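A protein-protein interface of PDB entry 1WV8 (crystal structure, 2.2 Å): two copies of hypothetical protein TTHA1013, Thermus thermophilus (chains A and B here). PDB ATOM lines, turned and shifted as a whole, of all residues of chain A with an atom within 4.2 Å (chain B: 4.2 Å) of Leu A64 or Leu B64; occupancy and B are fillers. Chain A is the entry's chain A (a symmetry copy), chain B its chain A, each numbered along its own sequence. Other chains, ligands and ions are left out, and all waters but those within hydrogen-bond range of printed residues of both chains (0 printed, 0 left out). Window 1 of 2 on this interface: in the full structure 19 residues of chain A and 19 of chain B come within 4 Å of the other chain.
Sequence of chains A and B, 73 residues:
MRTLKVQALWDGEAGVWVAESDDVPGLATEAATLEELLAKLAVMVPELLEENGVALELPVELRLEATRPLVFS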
ATOM      1  N   VAL A   6     -27.166 -12.035  -6.512  1.00  0.00           N
ATOM      2  CA  VAL A   6     -27.869 -13.020  -5.698  1.00  0.00           C
ATOM      3  C   VAL A   6     -28.027 -12.466  -4.287  1.00  0.00           C
ATOM      4  O   VAL A   6     -27.044 -12.044  -3.655  1.00  0.00           O
ATOM      5  CB  VAL A   6     -27.081 -14.342  -5.610  1.00  0.00           C
ATOM      6  CG1 VAL A   6     -27.796 -15.338  -4.685  1.00  0.00           C
ATOM      7  CG2 VAL A   6     -26.919 -14.927  -7.001  1.00  0.00           C
ATOM      8  N   GLN A   7     -29.258 -12.452  -3.784  1.00  0.00           N
ATOM      9  CA  GLN A   7     -29.480 -11.954  -2.437  1.00  0.00           C
ATOM     10  C   GLN A   7     -29.439 -13.078  -1.415  1.00  0.00           C
ATOM     11  O   GLN A   7     -29.926 -14.183  -1.664  1.00  0.00           O
ATOM     12  CB  GLN A   7     -30.816 -11.231  -2.317  1.00  0.00           C
ATOM     13  CG  GLN A   7     -30.909  -9.919  -3.053  1.00  0.00           C
ATOM     14  CD  GLN A   7     -31.249 -10.101  -4.512  1.00  0.00           C
ATOM     15  OE1 GLN A   7     -32.225 -10.763  -4.846  1.00  0.00           O
ATOM     16  NE2 GLN A   7     -30.450  -9.503  -5.393  1.00  0.00           N
ATOM     17  N   ALA A   8     -28.847 -12.781  -0.265  1.00  0.00           N
ATOM     18  CA  ALA A   8     -28.769 -13.734   0.830  1.00  0.00           C
ATOM     19  C   ALA A   8     -29.681 -13.120   1.868  1.00  0.00           C
ATOM     20  O   ALA A   8     -29.433 -12.009   2.334  1.00  0.00           O
ATOM     21  CB  ALA A   8     -27.352 -13.836   1.369  1.00  0.00           C
ATOM     22  N   LEU A  37     -22.724 -20.472   2.002  1.00  0.00           N
ATOM     23  CA  LEU A  37     -23.702 -20.119   0.983  1.00  0.00           C
ATOM     24  C   LEU A  37     -22.940 -19.797  -0.304  1.00  0.00           C
ATOM     25  O   LEU A  37     -23.371 -20.165  -1.402  1.00  0.00           O
ATOM     26  CB  LEU A  37     -24.501 -18.892   1.406  1.00  0.00           C
ATOM     27  CG  LEU A  37     -25.992 -18.781   1.051  1.00  0.00           C
ATOM     28  CD1 LEU A  37     -26.246 -17.351   0.695  1.00  0.00           C
ATOM     29  CD2 LEU A  37     -26.397 -19.670  -0.112  1.00  0.00           C
ATOM     30  N   LEU A  38     -21.810 -19.101  -0.169  1.00  0.00           N
ATOM     31  CA  LEU A  38     -20.999 -18.742  -1.336  1.00  0.00           C
ATOM     32  C   LEU A  38     -20.470 -20.000  -1.992  1.00  0.00           C
ATOM     33  O   LEU A  38     -20.587 -20.172  -3.198  1.00  0.00           O
ATOM     34  CB  LEU A  38     -19.814 -17.861  -0.942  1.00  0.00           C
ATOM     35  CG  LEU A  38     -19.999 -16.356  -1.133  1.00  0.00           C
ATOM     36  CD1 LEU A  38     -18.830 -15.610  -0.523  1.00  0.00           C
ATOM     37  CD2 LEU A  38     -20.133 -16.041  -2.613  1.00  0.00           C
ATOM     38  N   LEU A  41     -23.158 -21.792  -3.825  1.00  0.00           N
ATOM     39  CA  LEU A  41     -23.539 -21.041  -5.018  1.00  0.00           C
ATOM     40  C   LEU A  41     -22.570 -21.224  -6.188  1.00  0.00           C
ATOM     41  O   LEU A  41     -22.986 -21.343  -7.339  1.00  0.00           O
ATOM     42  CB  LEU A  41     -23.663 -19.551  -4.676  1.00  0.00           C
ATOM     43  CG  LEU A  41     -25.038 -19.031  -4.220  1.00  0.00           C
ATOM     44  CD1 LEU A  41     -25.746 -20.093  -3.434  1.00  0.00           C
ATOM     45  CD2 LEU A  41     -24.878 -17.762  -3.381  1.00  0.00           C
ATOM     46  N   LEU A  62     -20.251 -13.784  -9.702  1.00  0.00           N
ATOM     47  CA  LEU A  62     -21.381 -13.863  -8.784  1.00  0.00           C
ATOM     48  C   LEU A  62     -21.278 -12.796  -7.680  1.00  0.00           C
ATOM     49  O   LEU A  62     -20.283 -12.753  -6.958  1.00  0.00           O
ATOM     50  CB  LEU A  62     -21.398 -15.256  -8.150  1.00  0.00           C
ATOM     51  CG  LEU A  62     -22.466 -15.596  -7.116  1.00  0.00           C
ATOM     52  CD1 LEU A  62     -23.801 -15.757  -7.810  1.00  0.00           C
ATOM     53  CD2 LEU A  62     -22.082 -16.885  -6.403  1.00  0.00           C
ATOM     54  N   ARG A  63     -22.289 -11.931  -7.557  1.00  0.00           N
ATOM     55  CA  ARG A  63     -22.286 -10.906  -6.504  1.00  0.00           C
ATOM     56  C   ARG A  63     -23.317 -11.258  -5.415  1.00  0.00           C
ATOM     57  O   ARG A  63     -24.525 -11.067  -5.592  1.00  0.00           O
ATOM     58  CB  ARG A  63     -22.605  -9.519  -7.076  1.00  0.00           C
ATOM     59  CG  ARG A  63     -22.500  -8.393  -6.039  1.00  0.00           C
ATOM     60  CD  ARG A  63     -22.850  -7.023  -6.619  1.00  0.00           C
ATOM     61  NE  ARG A  63     -21.978  -6.625  -7.724  1.00  0.00           N
ATOM     62  CZ  ARG A  63     -22.109  -5.490  -8.408  1.00  0.00           C
ATOM     63  NH1 ARG A  63     -23.079  -4.639  -8.098  1.00  0.00           N
ATOM     64  NH2 ARG A  63     -21.283  -5.208  -9.408  1.00  0.00           N
ATOM     65  N   LEU A  64     -22.840 -11.798  -4.298  1.00  0.00           N
ATOM     66  CA  LEU A  64     -23.718 -12.153  -3.185  1.00  0.00           C
ATOM     67  C   LEU A  64     -23.956 -10.904  -2.346  1.00  0.00           C
ATOM     68  O   LEU A  64     -23.009 -10.301  -1.834  1.00  0.00           O
ATOM     69  CB  LEU A  64     -23.079 -13.219  -2.315  1.00  0.00           C
ATOM     70  CG  LEU A  64     -23.974 -14.321  -1.727  1.00  0.00           C
ATOM     71  CD1 LEU A  64     -23.389 -14.743  -0.392  1.00  0.00           C
ATOM     72  CD2 LEU A  64     -25.406 -13.849  -1.550  1.00  0.00           C
ATOM     73  N   GLU A  65     -25.223 -10.524  -2.207  1.00  0.00           N
ATOM     74  CA  GLU A  65     -25.597  -9.330  -1.458  1.00  0.00           C
ATOM     75  C   GLU A  65     -26.373  -9.643  -0.179  1.00  0.00           C
ATOM     76  O   GLU A  65     -27.289 -10.463  -0.181  1.00  0.00           O
ATOM     77  CB  GLU A  65     -26.440  -8.417  -2.351  1.00  0.00           C
ATOM     78  CG  GLU A  65     -25.739  -8.027  -3.656  1.00  0.00           C
ATOM     79  CD  GLU A  65     -26.692  -7.433  -4.681  1.00  0.00           C
ATOM     80  OE1 GLU A  65     -27.696  -8.106  -5.007  1.00  0.00           O
ATOM     81  OE2 GLU A  65     -26.435  -6.303  -5.164  1.00  0.00           O
ATOM     82  N   ALA A  66     -25.996  -8.985   0.910  1.00  0.00           N
ATOM     83  CA  ALA A  66     -26.659  -9.166   2.194  1.00  0.00           C
ATOM     84  C   ALA A  66     -26.958  -7.784   2.736  1.00  0.00           C
ATOM     85  O   ALA A  66     -26.042  -6.969   2.912  1.00  0.00           O
ATOM     86  CB  ALA A  66     -25.755  -9.926   3.168  1.00  0.00           C
ATOM     87  N   VAL B   6     -21.431  -1.553   0.279  1.00  0.00           N
ATOM     88  CA  VAL B   6     -20.123  -1.811   0.873  1.00  0.00           C
ATOM     89  C   VAL B   6     -19.592  -3.133   0.331  1.00  0.00           C
ATOM     90  O   VAL B   6     -20.277  -4.167   0.393  1.00  0.00           O
ATOM     91  CB  VAL B   6     -20.215  -1.921   2.407  1.00  0.00           C
ATOM     92  CG1 VAL B   6     -18.845  -2.272   3.007  1.00  0.00           C
ATOM     93  CG2 VAL B   6     -20.729  -0.613   2.978  1.00  0.00           C
ATOM     94  N   GLN B   7     -18.377  -3.113  -0.211  1.00  0.00           N
ATOM     95  CA  GLN B   7     -17.800  -4.341  -0.731  1.00  0.00           C
ATOM     96  C   GLN B   7     -16.953  -5.044   0.317  1.00  0.00           C
ATOM     97  O   GLN B   7     -16.239  -4.404   1.093  1.00  0.00           O
ATOM     98  CB  GLN B   7     -16.942  -4.082  -1.962  1.00  0.00           C
ATOM     99  CG  GLN B   7     -17.695  -3.655  -3.196  1.00  0.00           C
ATOM    100  CD  GLN B   7     -17.986  -2.174  -3.208  1.00  0.00           C
ATOM    101  OE1 GLN B   7     -17.084  -1.361  -3.046  1.00  0.00           O
ATOM    102  NE2 GLN B   7     -19.251  -1.814  -3.413  1.00  0.00           N
ATOM    103  N   ALA B   8     -17.046  -6.368   0.330  1.00  0.00           N
ATOM    104  CA  ALA B   8     -16.262  -7.186   1.241  1.00  0.00           C
ATOM    105  C   ALA B   8     -15.305  -7.893   0.309  1.00  0.00           C
ATOM    106  O   ALA B   8     -15.731  -8.637  -0.572  1.00  0.00           O
ATOM    107  CB  ALA B   8     -17.138  -8.197   1.962  1.00  0.00           C
ATOM    108  N   LEU B  37     -18.058  -9.184   9.964  1.00  0.00           N
ATOM    109  CA  LEU B  37     -17.846  -7.963   9.201  1.00  0.00           C
ATOM    110  C   LEU B  37     -19.152  -7.166   9.220  1.00  0.00           C
ATOM    111  O   LEU B  37     -19.140  -5.937   9.343  1.00  0.00           O
ATOM    112  CB  LEU B  37     -17.486  -8.288   7.756  1.00  0.00           C
ATOM    113  CG  LEU B  37     -16.473  -7.416   6.998  1.00  0.00           C
ATOM    114  CD1 LEU B  37     -16.974  -7.293   5.594  1.00  0.00           C
ATOM    115  CD2 LEU B  37     -16.310  -6.031   7.598  1.00  0.00           C
ATOM    116  N   LEU B  38     -20.280  -7.867   9.091  1.00  0.00           N
ATOM    117  CA  LEU B  38     -21.587  -7.206   9.102  1.00  0.00           C
ATOM    118  C   LEU B  38     -21.818  -6.560  10.452  1.00  0.00           C
ATOM    119  O   LEU B  38     -22.184  -5.395  10.533  1.00  0.00           O
ATOM    120  CB  LEU B  38     -22.717  -8.199   8.835  1.00  0.00           C
ATOM    121  CG  LEU B  38     -23.231  -8.266   7.397  1.00  0.00           C
ATOM    122  CD1 LEU B  38     -24.202  -9.420   7.249  1.00  0.00           C
ATOM    123  CD2 LEU B  38     -23.892  -6.948   7.028  1.00  0.00           C
ATOM    124  N   LEU B  41     -19.745  -3.505  10.855  1.00  0.00           N
ATOM    125  CA  LEU B  41     -20.247  -2.440   9.990  1.00  0.00           C
ATOM    126  C   LEU B  41     -21.475  -1.725  10.557  1.00  0.00           C
ATOM    127  O   LEU B  41     -21.594  -0.504  10.461  1.00  0.00           O
ATOM    128  CB  LEU B  41     -20.571  -3.007   8.602  1.00  0.00           C
ATOM    129  CG  LEU B  41     -19.456  -2.994   7.543  1.00  0.00           C
ATOM    130  CD1 LEU B  41     -18.127  -3.208   8.202  1.00  0.00           C
ATOM    131  CD2 LEU B  41     -19.709  -4.071   6.487  1.00  0.00           C
ATOM    132  N   LEU B  62     -27.767  -0.994   4.817  1.00  0.00           N
ATOM    133  CA  LEU B  62     -26.417  -1.367   4.410  1.00  0.00           C
ATOM    134  C   LEU B  62     -26.430  -2.619   3.516  1.00  0.00           C
ATOM    135  O   LEU B  62     -26.939  -3.662   3.927  1.00  0.00           O
ATOM    136  CB  LEU B  62     -25.589  -1.643   5.667  1.00  0.00           C
ATOM    137  CG  LEU B  62     -24.137  -2.091   5.525  1.00  0.00           C
ATOM    138  CD1 LEU B  62     -23.294  -0.918   5.073  1.00  0.00           C
ATOM    139  CD2 LEU B  62     -23.640  -2.614   6.865  1.00  0.00           C
ATOM    140  N   ARG B  63     -25.889  -2.518   2.299  1.00  0.00           N
ATOM    141  CA  ARG B  63     -25.827  -3.677   1.398  1.00  0.00           C
ATOM    142  C   ARG B  63     -24.377  -4.186   1.283  1.00  0.00           C
ATOM    143  O   ARG B  63     -23.548  -3.600   0.581  1.00  0.00           O
ATOM    144  CB  ARG B  63     -26.354  -3.326   0.001  1.00  0.00           C
ATOM    145  CG  ARG B  63     -26.420  -4.531  -0.947  1.00  0.00           C
ATOM    146  CD  ARG B  63     -26.917  -4.157  -2.342  1.00  0.00           C
ATOM    147  NE  ARG B  63     -28.263  -3.582  -2.339  1.00  0.00           N
ATOM    148  CZ  ARG B  63     -28.894  -3.150  -3.430  1.00  0.00           C
ATOM    149  NH1 ARG B  63     -28.299  -3.230  -4.613  1.00  0.00           N
ATOM    150  NH2 ARG B  63     -30.111  -2.628  -3.340  1.00  0.00           N
ATOM    151  N   LEU B  64     -24.067  -5.263   1.999  1.00  0.00           N
ATOM    152  CA  LEU B  64     -22.731  -5.852   1.954  1.00  0.00           C
ATOM    153  C   LEU B  64     -22.653  -6.772   0.743  1.00  0.00           C
ATOM    154  O   LEU B  64     -23.431  -7.722   0.624  1.00  0.00           O
ATOM    155  CB  LEU B  64     -22.458  -6.661   3.209  1.00  0.00           C
ATOM    156  CG  LEU B  64     -21.049  -6.617   3.819  1.00  0.00           C
ATOM    157  CD1 LEU B  64     -20.777  -7.956   4.478  1.00  0.00           C
ATOM    158  CD2 LEU B  64     -19.990  -6.320   2.771  1.00  0.00           C
ATOM    159  N   GLU B  65     -21.709  -6.486  -0.151  1.00  0.00           N
ATOM    160  CA  GLU B  65     -21.539  -7.261  -1.374  1.00  0.00           C
ATOM    161  C   GLU B  65     -20.229  -8.047  -1.408  1.00  0.00           C
ATOM    162  O   GLU B  65     -19.169  -7.523  -1.072  1.00  0.00           O
ATOM    163  CB  GLU B  65     -21.598  -6.321  -2.580  1.00  0.00           C
ATOM    164  CG  GLU B  65     -22.888  -5.499  -2.647  1.00  0.00           C
ATOM    165  CD  GLU B  65     -22.792  -4.332  -3.618  1.00  0.00           C
ATOM    166  OE1 GLU B  65     -21.859  -3.512  -3.457  1.00  0.00           O
ATOM    167  OE2 GLU B  65     -23.648  -4.230  -4.531  1.00  0.00           O
ATOM    168  N   ALA B  66     -20.313  -9.308  -1.815  1.00  0.00           N
ATOM    169  CA  ALA B  66     -19.143 -10.168  -1.918  1.00  0.00           C
ATOM    170  C   ALA B  66     -19.197 -10.825  -3.282  1.00  0.00           C
ATOM    171  O   ALA B  66     -20.178 -11.505  -3.611  1.00  0.00           O
ATOM    172  CB  ALA B  66     -19.157 -11.237  -0.822  1.00  0.00           C
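Arg A63 touches Glu B65, and with the chains exchanged Glu A65 touches Arg B63. Arg A63 touches Ala B66, and with the chains exchanged Ala A66 touches Arg B63. Leu A64 touches Ala B66, and with the chains exchanged Ala A66 touches Leu B64. Glu B65 touches its own counterpart, Glu A65. Of the 12 pairs that touch across the chains among the printed residues, 12 have their exchanged pair printed and touching as well.
The backbone carbonyl oxygen (O) of Arg B63 lies within hydrogen-bond range of the backbone NH (N) of Val B6, at 3.0 Å. The backbone NH (N) of Ala A8 sits at hydrogen-bond distance from the backbone carbonyl oxygen (O) of Glu A65 (2.8 Å). NE2 of Gln B7 sits at hydrogen-bond distance from OE1 of Glu B65. N of Glu A65 lies within hydrogen-bond range of O of Val A6 (2.8 Å). The backbone NH (N) of Ala B8 sits at hydrogen-bond distance from the backbone carbonyl oxygen (O) of Glu B65, at 2.8 Å. The side-chain carboxylate of Glu A65 sits at hydrogen-bond distance from the side-chain amide nitrogen of Gln A7 (3.1 Å).
Among the printed residues, merely in contact across the chains: Leu A62 with Ala B66 (3.6 Å), Arg A63 with Ala B66 (3.6 Å), Leu A64 with Leu B64 (3.6 Å), Leu A64 with Glu B65 (3.4 Å), Glu A65 with Leu B64 (3.4 Å), Glu A65 with Glu B65 (3.5 Å), Ala A66 with Leu B62 (3.6 Å) and Ala A66 with Arg B63 (3.6 Å).
Val A6 touches none of the printed residues of chain B. Ala A8 touches none of the printed residues of chain B. Printed residues of chain B within 4 Å of Leu A64: Leu B64 (3.6 Å), Glu B65 (3.4 Å) and Ala B66 (2.8 Å). Of the printed residues of chain A, Leu B62 touches Ala A66 (3.6 Å). Of the printed residues of chain A, Arg B63 touches Glu A65 (3.6 Å) and Ala A66 (3.6 Å). Leu B64 touches just these residues of chain A: Leu A64 (3.6 Å), Glu A65 (3.4 Å) and Ala A66 (2.8 Å). The nearest printed residue of chain A that does not touch Leu B64 is Arg A63 (6.8 Å).
Of the 11 printed residues of chain A, 5 touch a printed residue of chain B. Printed residues of chain A that touch a printed residue of chain B: Leu A62, Arg A63, Leu A64, Glu A65 and Ala A66. Hydrophobic or aromatic side chains of chain A that line the printed part of chain B: Leu A64. Among the printed residues, Asp or Glu carboxylates within 4 Å of a Lys or Arg side-chain nitrogen of the other chain: Arg A63 with Glu B65 and Glu A65 with Arg B63.
OE2 of Glu B65 lies within salt-bridge range of NH1 of Arg A63 (3.6 Å). The backbone carbonyl oxygen (O) of Ala B66 sits at hydrogen-bond distance from the backbone NH (N) of Leu A64. N of Leu B64 is in hydrogen-bond range of O of Ala A66 (2.8 Å). The side-chain carboxylate (OE2) of Glu A65 is in salt-bridge range of the guanidinium group (NH1) of Arg B63 (3.6 Å).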
